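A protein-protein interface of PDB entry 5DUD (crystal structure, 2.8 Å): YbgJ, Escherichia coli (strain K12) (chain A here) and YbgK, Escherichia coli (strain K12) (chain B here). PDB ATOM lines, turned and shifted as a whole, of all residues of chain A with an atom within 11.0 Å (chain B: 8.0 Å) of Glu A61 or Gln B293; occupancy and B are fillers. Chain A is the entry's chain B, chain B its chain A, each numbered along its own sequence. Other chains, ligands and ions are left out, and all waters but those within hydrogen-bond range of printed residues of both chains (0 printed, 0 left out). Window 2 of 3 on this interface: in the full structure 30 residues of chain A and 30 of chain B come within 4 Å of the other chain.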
ATOM      1  N   LEU A   8      -2.502  21.880  -6.443  1.00  0.00           N
ATOM      2  CA  LEU A   8      -1.588  22.594  -7.315  1.00  0.00           C
ATOM      3  C   LEU A   8      -2.391  23.199  -8.438  1.00  0.00           C
ATOM      4  O   LEU A   8      -3.249  22.512  -8.994  1.00  0.00           O
ATOM      5  CB  LEU A   8      -0.458  21.704  -7.872  1.00  0.00           C
ATOM      6  CG  LEU A   8       0.712  21.366  -6.944  1.00  0.00           C
ATOM      7  CD1 LEU A   8       1.825  20.688  -7.715  1.00  0.00           C
ATOM      8  CD2 LEU A   8       1.284  22.605  -6.252  1.00  0.00           C
ATOM      9  N   GLY A  10      -1.585  24.498 -11.770  1.00  0.00           N
ATOM     10  CA  GLY A  10      -0.500  24.508 -12.732  1.00  0.00           C
ATOM     11  C   GLY A  10       0.770  24.093 -12.022  1.00  0.00           C
ATOM     12  O   GLY A  10       0.712  23.431 -10.985  1.00  0.00           O
ATOM     13  N   GLU A  11       1.918  24.515 -12.539  1.00  0.00           N
ATOM     14  CA  GLU A  11       3.204  24.180 -11.935  1.00  0.00           C
ATOM     15  C   GLU A  11       3.834  25.387 -11.224  1.00  0.00           C
ATOM     16  O   GLU A  11       4.959  25.256 -10.758  1.00  0.00           O
ATOM     17  CB  GLU A  11       4.157  23.588 -13.003  1.00  0.00           C
ATOM     18  CG  GLU A  11       4.960  24.536 -13.893  1.00  0.00           C
ATOM     19  CD  GLU A  11       4.213  25.426 -14.870  1.00  0.00           C
ATOM     20  OE1 GLU A  11       3.028  25.741 -14.618  1.00  0.00           O
ATOM     21  OE2 GLU A  11       4.837  25.846 -15.871  1.00  0.00           O
ATOM     22  N   THR A  12       3.115  26.528 -11.094  1.00  0.00           N
ATOM     23  CA  THR A  12       3.666  27.740 -10.477  1.00  0.00           C
ATOM     24  C   THR A  12       2.865  28.271  -9.276  1.00  0.00           C
ATOM     25  O   THR A  12       3.335  29.223  -8.653  1.00  0.00           O
ATOM     26  CB  THR A  12       3.776  28.843 -11.547  1.00  0.00           C
ATOM     27  N   ALA A  13       1.693  27.693  -8.941  1.00  0.00           N
ATOM     28  CA  ALA A  13       0.892  28.162  -7.823  1.00  0.00           C
ATOM     29  C   ALA A  13       0.269  27.006  -7.072  1.00  0.00           C
ATOM     30  O   ALA A  13       0.249  25.890  -7.571  1.00  0.00           O
ATOM     31  CB  ALA A  13      -0.181  29.095  -8.341  1.00  0.00           C
ATOM     32  N   PRO A  41      11.123  36.516  -0.175  1.00  0.00           N
ATOM     33  CA  PRO A  41      11.534  36.569  -1.596  1.00  0.00           C
ATOM     34  C   PRO A  41      10.948  35.514  -2.540  1.00  0.00           C
ATOM     35  O   PRO A  41      10.799  35.813  -3.722  1.00  0.00           O
ATOM     36  CB  PRO A  41      13.054  36.366  -1.517  1.00  0.00           C
ATOM     37  CG  PRO A  41      13.429  36.729  -0.148  1.00  0.00           C
ATOM     38  CD  PRO A  41      12.293  36.301   0.701  1.00  0.00           C
ATOM     39  N   ASN A  42      10.642  34.299  -2.064  1.00  0.00           N
ATOM     40  CA  ASN A  42      10.169  33.209  -2.941  1.00  0.00           C
ATOM     41  C   ASN A  42       8.688  33.295  -3.420  1.00  0.00           C
ATOM     42  O   ASN A  42       8.316  32.515  -4.299  1.00  0.00           O
ATOM     43  CB  ASN A  42      10.379  31.862  -2.250  1.00  0.00           C
ATOM     44  N   VAL A  44       6.038  35.434  -5.416  1.00  0.00           N
ATOM     45  CA  VAL A  44       5.796  36.540  -6.342  1.00  0.00           C
ATOM     46  C   VAL A  44       4.469  37.251  -6.001  1.00  0.00           C
ATOM     47  O   VAL A  44       4.440  38.479  -5.966  1.00  0.00           O
ATOM     48  CB  VAL A  44       5.852  36.125  -7.842  1.00  0.00           C
ATOM     49  CG1 VAL A  44       7.191  35.499  -8.193  1.00  0.00           C
ATOM     50  CG2 VAL A  44       4.710  35.186  -8.252  1.00  0.00           C
ATOM     51  N   ILE A  56       1.329  32.253  -5.740  1.00  0.00           N
ATOM     52  CA  ILE A  56       2.183  31.987  -6.898  1.00  0.00           C
ATOM     53  C   ILE A  56       3.620  32.002  -6.385  1.00  0.00           C
ATOM     54  O   ILE A  56       3.936  32.815  -5.522  1.00  0.00           O
ATOM     55  CB  ILE A  56       1.926  32.978  -8.059  1.00  0.00           C
ATOM     56  N   LEU A  57       4.486  31.099  -6.898  1.00  0.00           N
ATOM     57  CA  LEU A  57       5.880  30.963  -6.442  1.00  0.00           C
ATOM     58  C   LEU A  57       6.908  31.346  -7.508  1.00  0.00           C
ATOM     59  O   LEU A  57       6.687  31.092  -8.689  1.00  0.00           O
ATOM     60  CB  LEU A  57       6.151  29.505  -6.021  1.00  0.00           C
ATOM     61  CG  LEU A  57       5.224  28.931  -4.928  1.00  0.00           C
ATOM     62  CD1 LEU A  57       5.133  27.464  -5.015  1.00  0.00           C
ATOM     63  CD2 LEU A  57       5.628  29.340  -3.486  1.00  0.00           C
ATOM     64  N   ARG A  58       8.058  31.896  -7.070  1.00  0.00           N
ATOM     65  CA  ARG A  58       9.154  32.302  -7.951  1.00  0.00           C
ATOM     66  C   ARG A  58      10.116  31.124  -8.216  1.00  0.00           C
ATOM     67  O   ARG A  58      10.789  31.125  -9.249  1.00  0.00           O
ATOM     68  CB  ARG A  58       9.922  33.487  -7.346  1.00  0.00           C
ATOM     69  CG  ARG A  58      10.524  34.430  -8.391  1.00  0.00           C
ATOM     70  CD  ARG A  58      11.451  35.472  -7.780  1.00  0.00           C
ATOM     71  NE  ARG A  58      10.822  36.224  -6.691  1.00  0.00           N
ATOM     72  CZ  ARG A  58       9.994  37.258  -6.824  1.00  0.00           C
ATOM     73  NH1 ARG A  58       9.649  37.688  -8.041  1.00  0.00           N
ATOM     74  NH2 ARG A  58       9.483  37.855  -5.754  1.00  0.00           N
ATOM     75  N   ASN A  59      10.193  30.141  -7.288  1.00  0.00           N
ATOM     76  CA  ASN A  59      11.043  28.945  -7.414  1.00  0.00           C
ATOM     77  C   ASN A  59      10.179  27.661  -7.282  1.00  0.00           C
ATOM     78  O   ASN A  59      10.336  26.886  -6.330  1.00  0.00           O
ATOM     79  CB  ASN A  59      12.169  28.985  -6.374  1.00  0.00           C
ATOM     80  N   PRO A  60       9.268  27.435  -8.261  1.00  0.00           N
ATOM     81  CA  PRO A  60       8.366  26.277  -8.190  1.00  0.00           C
ATOM     82  C   PRO A  60       9.053  24.929  -8.350  1.00  0.00           C
ATOM     83  O   PRO A  60       8.546  23.962  -7.811  1.00  0.00           O
ATOM     84  CB  PRO A  60       7.384  26.513  -9.341  1.00  0.00           C
ATOM     85  CG  PRO A  60       8.095  27.385 -10.279  1.00  0.00           C
ATOM     86  CD  PRO A  60       8.965  28.259  -9.443  1.00  0.00           C
ATOM     87  N   GLU A  61      10.186  24.843  -9.062  1.00  0.00           N
ATOM     88  CA  GLU A  61      10.876  23.564  -9.256  1.00  0.00           C
ATOM     89  C   GLU A  61      11.237  22.894  -7.918  1.00  0.00           C
ATOM     90  O   GLU A  61      11.177  21.668  -7.835  1.00  0.00           O
ATOM     91  CB  GLU A  61      12.130  23.719 -10.146  1.00  0.00           C
ATOM     92  CG  GLU A  61      13.359  24.388  -9.533  1.00  0.00           C
ATOM     93  CD  GLU A  61      13.261  25.872  -9.236  1.00  0.00           C
ATOM     94  OE1 GLU A  61      13.747  26.297  -8.162  1.00  0.00           O
ATOM     95  OE2 GLU A  61      12.697  26.612 -10.074  1.00  0.00           O
ATOM     96  N   SER A  62      11.606  23.668  -6.891  1.00  0.00           N
ATOM     97  CA  SER A  62      11.942  23.100  -5.585  1.00  0.00           C
ATOM     98  C   SER A  62      10.732  23.119  -4.673  1.00  0.00           C
ATOM     99  O   SER A  62      10.448  22.134  -3.996  1.00  0.00           O
ATOM    100  CB  SER A  62      13.096  23.868  -4.932  1.00  0.00           C
ATOM    101  OG  SER A  62      13.610  24.896  -5.763  1.00  0.00           O
ATOM    102  N   LEU A  63      10.026  24.246  -4.661  1.00  0.00           N
ATOM    103  CA  LEU A  63       8.945  24.491  -3.728  1.00  0.00           C
ATOM    104  C   LEU A  63       7.627  23.838  -4.090  1.00  0.00           C
ATOM    105  O   LEU A  63       6.745  23.905  -3.248  1.00  0.00           O
ATOM    106  CB  LEU A  63       8.717  26.022  -3.596  1.00  0.00           C
ATOM    107  CG  LEU A  63       9.787  26.865  -2.821  1.00  0.00           C
ATOM    108  CD1 LEU A  63      11.222  26.347  -2.975  1.00  0.00           C
ATOM    109  CD2 LEU A  63       9.725  28.340  -3.209  1.00  0.00           C
ATOM    110  N   ALA A  64       7.440  23.254  -5.288  1.00  0.00           N
ATOM    111  CA  ALA A  64       6.122  22.719  -5.683  1.00  0.00           C
ATOM    112  C   ALA A  64       5.515  21.673  -4.699  1.00  0.00           C
ATOM    113  O   ALA A  64       4.440  21.910  -4.141  1.00  0.00           O
ATOM    114  CB  ALA A  64       6.186  22.125  -7.085  1.00  0.00           C
ATOM    115  N   LEU A  65       6.176  20.528  -4.510  1.00  0.00           N
ATOM    116  CA  LEU A  65       5.668  19.478  -3.597  1.00  0.00           C
ATOM    117  C   LEU A  65       5.617  19.966  -2.128  1.00  0.00           C
ATOM    118  O   LEU A  65       4.675  19.636  -1.387  1.00  0.00           O
ATOM    119  CB  LEU A  65       6.512  18.189  -3.710  1.00  0.00           C
ATOM    120  CG  LEU A  65       8.006  18.292  -3.343  1.00  0.00           C
ATOM    121  CD1 LEU A  65       8.276  17.770  -1.939  1.00  0.00           C
ATOM    122  CD2 LEU A  65       8.874  17.539  -4.341  1.00  0.00           C
ATOM    123  N   ASP A  66       6.610  20.799  -1.749  1.00  0.00           N
ATOM    124  CA  ASP A  66       6.724  21.410  -0.420  1.00  0.00           C
ATOM    125  C   ASP A  66       5.515  22.300  -0.136  1.00  0.00           C
ATOM    126  O   ASP A  66       5.074  22.363   1.003  1.00  0.00           O
ATOM    127  CB  ASP A  66       8.014  22.242  -0.309  1.00  0.00           C
ATOM    128  N   ALA A  67       4.968  22.960  -1.188  1.00  0.00           N
ATOM    129  CA  ALA A  67       3.795  23.841  -1.116  1.00  0.00           C
ATOM    130  C   ALA A  67       2.532  23.120  -0.648  1.00  0.00           C
ATOM    131  O   ALA A  67       1.631  23.795  -0.147  1.00  0.00           O
ATOM    132  CB  ALA A  67       3.519  24.460  -2.475  1.00  0.00           C
ATOM    133  N   ARG A  70       3.641  22.519   3.276  1.00  0.00           N
ATOM    134  CA  ARG A  70       3.957  23.789   3.965  1.00  0.00           C
ATOM    135  C   ARG A  70       2.758  24.753   4.155  1.00  0.00           C
ATOM    136  O   ARG A  70       2.650  25.338   5.230  1.00  0.00           O
ATOM    137  CB  ARG A  70       5.051  24.524   3.164  1.00  0.00           C
ATOM    138  CG  ARG A  70       5.830  25.653   3.856  1.00  0.00           C
ATOM    139  CD  ARG A  70       6.118  26.849   2.955  1.00  0.00           C
ATOM    140  NE  ARG A  70       6.551  26.489   1.603  1.00  0.00           N
ATOM    141  CZ  ARG A  70       6.877  27.359   0.651  1.00  0.00           C
ATOM    142  NH1 ARG A  70       6.841  28.669   0.897  1.00  0.00           N
ATOM    143  NH2 ARG A  70       7.243  26.938  -0.549  1.00  0.00           N
ATOM    144  N   ALA B 264       5.891  27.119 -20.338  1.00  0.00           N
ATOM    145  CA  ALA B 264       6.797  26.849 -21.460  1.00  0.00           C
ATOM    146  C   ALA B 264       6.058  26.776 -22.813  1.00  0.00           C
ATOM    147  O   ALA B 264       6.690  27.012 -23.839  1.00  0.00           O
ATOM    148  CB  ALA B 264       7.556  25.548 -21.218  1.00  0.00           C
ATOM    149  N   LEU B 285       3.844  16.942 -13.910  1.00  0.00           N
ATOM    150  CA  LEU B 285       4.474  18.024 -13.152  1.00  0.00           C
ATOM    151  C   LEU B 285       5.995  18.085 -13.396  1.00  0.00           C
ATOM    152  O   LEU B 285       6.521  19.187 -13.538  1.00  0.00           O
ATOM    153  CB  LEU B 285       4.162  17.888 -11.646  1.00  0.00           C
ATOM    154  CG  LEU B 285       4.425  19.114 -10.772  1.00  0.00           C
ATOM    155  CD1 LEU B 285       3.505  20.270 -11.138  1.00  0.00           C
ATOM    156  CD2 LEU B 285       4.265  18.777  -9.295  1.00  0.00           C
ATOM    157  N   GLU B 286       6.689  16.928 -13.476  1.00  0.00           N
ATOM    158  CA  GLU B 286       8.136  16.895 -13.748  1.00  0.00           C
ATOM    159  C   GLU B 286       8.412  17.377 -15.168  1.00  0.00           C
ATOM    160  O   GLU B 286       9.384  18.099 -15.388  1.00  0.00           O
ATOM    161  CB  GLU B 286       8.710  15.477 -13.538  1.00  0.00           C
ATOM    162  CG  GLU B 286      10.174  15.288 -13.931  1.00  0.00           C
ATOM    163  CD  GLU B 286      11.160  16.318 -13.412  1.00  0.00           C
ATOM    164  OE1 GLU B 286      11.005  16.768 -12.254  1.00  0.00           O
ATOM    165  OE2 GLU B 286      12.098  16.667 -14.165  1.00  0.00           O
ATOM    166  N   GLU B 287       7.522  17.041 -16.107  1.00  0.00           N
ATOM    167  CA  GLU B 287       7.664  17.478 -17.494  1.00  0.00           C
ATOM    168  C   GLU B 287       7.381  18.979 -17.598  1.00  0.00           C
ATOM    169  O   GLU B 287       8.114  19.700 -18.274  1.00  0.00           O
ATOM    170  CB  GLU B 287       6.730  16.691 -18.428  1.00  0.00           C
ATOM    171  CG  GLU B 287       6.923  15.185 -18.394  1.00  0.00           C
ATOM    172  CD  GLU B 287       5.991  14.412 -19.311  1.00  0.00           C
ATOM    173  OE1 GLU B 287       5.773  13.208 -19.049  1.00  0.00           O
ATOM    174  OE2 GLU B 287       5.445  15.015 -20.265  1.00  0.00           O
ATOM    175  N   ALA B 288       6.354  19.455 -16.883  1.00  0.00           N
ATOM    176  CA  ALA B 288       5.993  20.868 -16.864  1.00  0.00           C
ATOM    177  C   ALA B 288       7.100  21.739 -16.268  1.00  0.00           C
ATOM    178  O   ALA B 288       7.284  22.863 -16.730  1.00  0.00           O
ATOM    179  CB  ALA B 288       4.710  21.060 -16.076  1.00  0.00           C
ATOM    180  N   LEU B 289       7.797  21.238 -15.228  1.00  0.00           N
ATOM    181  CA  LEU B 289       8.878  21.959 -14.550  1.00  0.00           C
ATOM    182  C   LEU B 289      10.193  21.883 -15.326  1.00  0.00           C
ATOM    183  O   LEU B 289      10.917  22.878 -15.357  1.00  0.00           O
ATOM    184  CB  LEU B 289       9.080  21.427 -13.123  1.00  0.00           C
ATOM    185  CG  LEU B 289       7.964  21.777 -12.139  1.00  0.00           C
ATOM    186  CD1 LEU B 289       7.946  20.814 -10.961  1.00  0.00           C
ATOM    187  CD2 LEU B 289       8.035  23.246 -11.694  1.00  0.00           C
ATOM    188  N   LYS B 290      10.513  20.724 -15.943  1.00  0.00           N
ATOM    189  CA  LYS B 290      11.732  20.581 -16.752  1.00  0.00           C
ATOM    190  C   LYS B 290      11.607  21.427 -18.024  1.00  0.00           C
ATOM    191  O   LYS B 290      12.585  22.043 -18.442  1.00  0.00           O
ATOM    192  CB  LYS B 290      12.005  19.110 -17.107  1.00  0.00           C
ATOM    193  N   ALA B 291      10.392  21.485 -18.616  1.00  0.00           N
ATOM    194  CA  ALA B 291      10.121  22.304 -19.804  1.00  0.00           C
ATOM    195  C   ALA B 291      10.230  23.797 -19.479  1.00  0.00           C
ATOM    196  O   ALA B 291      10.666  24.573 -20.330  1.00  0.00           O
ATOM    197  CB  ALA B 291       8.738  21.993 -20.354  1.00  0.00           C
ATOM    198  N   ARG B 292       9.833  24.195 -18.251  1.00  0.00           N
ATOM    199  CA  ARG B 292       9.931  25.584 -17.787  1.00  0.00           C
ATOM    200  C   ARG B 292      11.399  25.959 -17.577  1.00  0.00           C
ATOM    201  O   ARG B 292      11.792  27.079 -17.906  1.00  0.00           O
ATOM    202  CB  ARG B 292       9.135  25.796 -16.486  1.00  0.00           C
ATOM    203  CG  ARG B 292       8.745  27.250 -16.239  1.00  0.00           C
ATOM    204  CD  ARG B 292       9.007  27.705 -14.814  1.00  0.00           C
ATOM    205  NE  ARG B 292       8.279  28.938 -14.493  1.00  0.00           N
ATOM    206  CZ  ARG B 292       8.470  29.677 -13.402  1.00  0.00           C
ATOM    207  NH1 ARG B 292       9.383  29.333 -12.501  1.00  0.00           N
ATOM    208  NH2 ARG B 292       7.750  30.778 -13.209  1.00  0.00           N
ATOM    209  N   GLN B 293      12.211  25.019 -17.039  1.00  0.00           N
ATOM    210  CA  GLN B 293      13.647  25.237 -16.848  1.00  0.00           C
ATOM    211  C   GLN B 293      14.328  25.381 -18.201  1.00  0.00           C
ATOM    212  O   GLN B 293      14.956  26.404 -18.449  1.00  0.00           O
ATOM    213  CB  GLN B 293      14.304  24.090 -16.054  1.00  0.00           C
ATOM    214  CG  GLN B 293      14.039  24.133 -14.552  1.00  0.00           C
ATOM    215  CD  GLN B 293      14.346  22.838 -13.819  1.00  0.00           C
ATOM    216  OE1 GLN B 293      13.677  22.498 -12.840  1.00  0.00           O
ATOM    217  NE2 GLN B 293      15.363  22.082 -14.232  1.00  0.00           N
ATOM    218  N   ASP B 294      14.142  24.394 -19.101  1.00  0.00           N
ATOM    219  CA  ASP B 294      14.722  24.390 -20.455  1.00  0.00           C
ATOM    220  C   ASP B 294      14.533  25.734 -21.185  1.00  0.00           C
ATOM    221  O   ASP B 294      15.458  26.178 -21.865  1.00  0.00           O
ATOM    222  CB  ASP B 294      14.116  23.258 -21.309  1.00  0.00           C
ATOM    223  CG  ASP B 294      14.539  21.847 -20.924  1.00  0.00           C
ATOM    224  OD1 ASP B 294      15.362  21.704 -19.991  1.00  0.00           O
ATOM    225  OD2 ASP B 294      14.027  20.887 -21.536  1.00  0.00           O
ATOM    226  N   GLN B 295      13.364  26.390 -21.021  1.00  0.00           N
ATOM    227  CA  GLN B 295      13.098  27.690 -21.643  1.00  0.00           C
ATOM    228  C   GLN B 295      13.804  28.814 -20.866  1.00  0.00           C
ATOM    229  O   GLN B 295      14.349  29.721 -21.488  1.00  0.00           O
ATOM    230  CB  GLN B 295      11.593  27.963 -21.752  1.00  0.00           C
ATOM    231  CG  GLN B 295      11.261  28.999 -22.821  1.00  0.00           C
ATOM    232  CD  GLN B 295       9.779  29.133 -23.047  1.00  0.00           C
ATOM    233  OE1 GLN B 295       9.218  28.550 -23.979  1.00  0.00           O
ATOM    234  NE2 GLN B 295       9.111  29.917 -22.214  1.00  0.00           N
ATOM    235  N   GLN B 296      13.862  28.724 -19.517  1.00  0.00           N
ATOM    236  CA  GLN B 296      14.614  29.692 -18.696  1.00  0.00           C
ATOM    237  C   GLN B 296      16.123  29.537 -18.950  1.00  0.00           C
ATOM    238  O   GLN B 296      16.852  30.526 -19.002  1.00  0.00           O
ATOM    239  CB  GLN B 296      14.308  29.528 -17.196  1.00  0.00           C
ATOM    240  CG  GLN B 296      12.977  30.146 -16.777  1.00  0.00           C
ATOM    241  CD  GLN B 296      12.718  30.019 -15.290  1.00  0.00           C
ATOM    242  OE1 GLN B 296      13.182  29.084 -14.625  1.00  0.00           O
ATOM    243  NE2 GLN B 296      11.941  30.941 -14.734  1.00  0.00           N
ATOM    244  N   ARG B 297      16.571  28.281 -19.119  1.00  0.00           N
ATOM    245  CA  ARG B 297      17.953  27.906 -19.426  1.00  0.00           C
ATOM    246  C   ARG B 297      18.339  28.342 -20.849  1.00  0.00           C
ATOM    247  O   ARG B 297      19.509  28.620 -21.107  1.00  0.00           O
ATOM    248  CB  ARG B 297      18.125  26.381 -19.283  1.00  0.00           C
ATOM    249  CG  ARG B 297      18.025  25.872 -17.839  1.00  0.00           C
ATOM    250  CD  ARG B 297      18.050  24.349 -17.759  1.00  0.00           C
ATOM    251  NE  ARG B 297      18.219  23.877 -16.384  1.00  0.00           N
ATOM    252  CZ  ARG B 297      18.466  22.618 -16.024  1.00  0.00           C
ATOM    253  NH1 ARG B 297      18.576  21.664 -16.950  1.00  0.00           N
ATOM    254  NH2 ARG B 297      18.594  22.295 -14.744  1.00  0.00           N
ATOM    255  N   TYR B 298      17.360  28.365 -21.772  1.00  0.00           N
ATOM    256  CA  TYR B 298      17.553  28.781 -23.164  1.00  0.00           C
ATOM    257  C   TYR B 298      17.882  30.293 -23.260  1.00  0.00           C
ATOM    258  O   TYR B 298      18.708  30.657 -24.089  1.00  0.00           O
ATOM    259  CB  TYR B 298      16.304  28.416 -24.003  1.00  0.00           C
ATOM    260  CG  TYR B 298      16.247  29.024 -25.385  1.00  0.00           C
ATOM    261  CD1 TYR B 298      16.965  28.472 -26.440  1.00  0.00           C
ATOM    262  CD2 TYR B 298      15.395  30.087 -25.664  1.00  0.00           C
ATOM    263  CE1 TYR B 298      16.879  28.999 -27.726  1.00  0.00           C
ATOM    264  CE2 TYR B 298      15.304  30.624 -26.944  1.00  0.00           C
ATOM    265  CZ  TYR B 298      16.056  30.083 -27.971  1.00  0.00           C
ATOM    266  OH  TYR B 298      15.961  30.601 -29.238  1.00  0.00           O
ATOM    267  N   PHE B 299      17.289  31.159 -22.406  1.00  0.00           N
ATOM    268  CA  PHE B 299      17.595  32.604 -22.434  1.00  0.00           C
ATOM    269  C   PHE B 299      19.012  32.893 -21.878  1.00  0.00           C
ATOM    270  O   PHE B 299      19.611  33.902 -22.248  1.00  0.00           O
ATOM    271  CB  PHE B 299      16.543  33.424 -21.663  1.00  0.00           C
ATOM    272  CG  PHE B 299      15.128  33.256 -22.173  1.00  0.00           C
ATOM    273  CD1 PHE B 299      14.791  33.615 -23.471  1.00  0.00           C
ATOM    274  CD2 PHE B 299      14.129  32.763 -21.347  1.00  0.00           C
ATOM    275  CE1 PHE B 299      13.489  33.444 -23.943  1.00  0.00           C
ATOM    276  CE2 PHE B 299      12.835  32.572 -21.828  1.00  0.00           C
ATOM    277  CZ  PHE B 299      12.519  32.930 -23.115  1.00  0.00           C
ATOM    278  N   GLU B 300      19.540  32.013 -21.000  1.00  0.00           N
ATOM    279  CA  GLU B 300      20.898  32.108 -20.449  1.00  0.00           C
ATOM    280  C   GLU B 300      21.925  31.742 -21.536  1.00  0.00           C
ATOM    281  O   GLU B 300      23.032  32.281 -21.525  1.00  0.00           O
ATOM    282  CB  GLU B 300      21.057  31.229 -19.197  1.00  0.00           C
ATOM    283  CG  GLU B 300      20.240  31.763 -18.032  1.00  0.00           C
ATOM    284  CD  GLU B 300      20.467  31.072 -16.703  1.00  0.00           C
ATOM    285  OE1 GLU B 300      20.205  29.852 -16.614  1.00  0.00           O
ATOM    286  OE2 GLU B 300      20.860  31.764 -15.735  1.00  0.00           O
ATOM    287  N   GLN B 301      21.551  30.858 -22.491  1.00  0.00           N
ATOM    288  CA  GLN B 301      22.398  30.528 -23.648  1.00  0.00           C
ATOM    289  C   GLN B 301      22.490  31.750 -24.577  1.00  0.00           C
ATOM    290  O   GLN B 301      23.568  32.041 -25.096  1.00  0.00           O
ATOM    291  CB  GLN B 301      21.865  29.308 -24.423  1.00  0.00           C
ATOM    292  CG  GLN B 301      22.143  27.964 -23.752  1.00  0.00           C
ATOM    293  CD  GLN B 301      21.020  26.966 -23.939  1.00  0.00           C
ATOM    294  OE1 GLN B 301      20.531  26.368 -22.975  1.00  0.00           O
ATOM    295  NE2 GLN B 301      20.585  26.747 -25.177  1.00  0.00           N
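NH2 of Arg B297 sits close to NE2 of Gln B293 (3.3 Å).
The guanidinium group (NE) of Arg A58 sits at hydrogen-bond distance from the backbone carbonyl oxygen (O) of Pro A41, at 3.0 Å.
The backbone carbonyl oxygen of Asn A42 sits at hydrogen-bond distance from the backbone NH of Arg A58 (2.9 Å).
The side-chain carboxylate (OE1) of Glu A61 sits at hydrogen-bond distance from the side-chain hydroxyl (OG) of Ser A62.
Among the printed residues, merely in contact across the chains: Pro A60 with Arg B292, Glu A61 with Gln B293, Leu A8 with Leu B285, Glu A61 with Leu B289, Glu A11 with Leu B289, Glu A11 with Leu B285, Pro A60 with Leu B289, Glu A11 with Ala B288 and Arg A58 with Arg B292.
Of chain B, only Leu B289 and Gln B293 come within 4 Å of Glu A61.
Of chain A, only Glu A61 (3.3 Å) comes within 4 Å of Gln B293.
Leu B289 touches three residues of chain A.
No residue of chain A comes within 4 Å of Lys B290.
No residue of chain A comes within 4 Å of Gln B296.
No residue of chain A comes within 4 Å of Arg B297.
Printed residues of chain B within 4 Å of Glu A11: Leu B285 (3.9 Å), Ala B288 (3.95 Å) and Leu B289 (3.8 Å).
Of the printed residues of chain A, Leu B285 touches Leu A8 and Glu A11.
Of the printed residues of chain B, Leu A8 touches Leu B285.
Of the printed residues of chain B, Arg A58 touches Arg B292.
Glu B287 touches none of the printed residues of chain A.
The nearest residue of chain B that does not touch Glu A61 is Arg B292 (4.9 Å).
The nearest residue of chain A that does not touch Gln B293 is Ser A62 (6.4 Å).
Of the 18 printed residues of chain B, 5 touch a printed residue of chain A.
Printed residues of chain B that touch a printed residue of chain A: Leu B285, Ala B288, Leu B289, Arg B292 and Gln B293.
Hydrophobic or aromatic side chains of chain B that line the printed part of chain A: Leu B285 and Leu B289.
Of the 21 printed residues of chain A, 5 touch a printed residue of chain B.
Printed residues of chain A that touch a printed residue of chain B: Leu A8, Glu A11, Arg A58, Pro A60 and Glu A61.
Along chain A the printed residues that touch a printed residue of chain B span positions 8 to 61.
Among the printed residues, 9 pairs touch across the chains.
Among the printed residues, no Asp or Glu carboxylate lies within 4 Å of a Lys or Arg side-chain nitrogen of the other chain.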
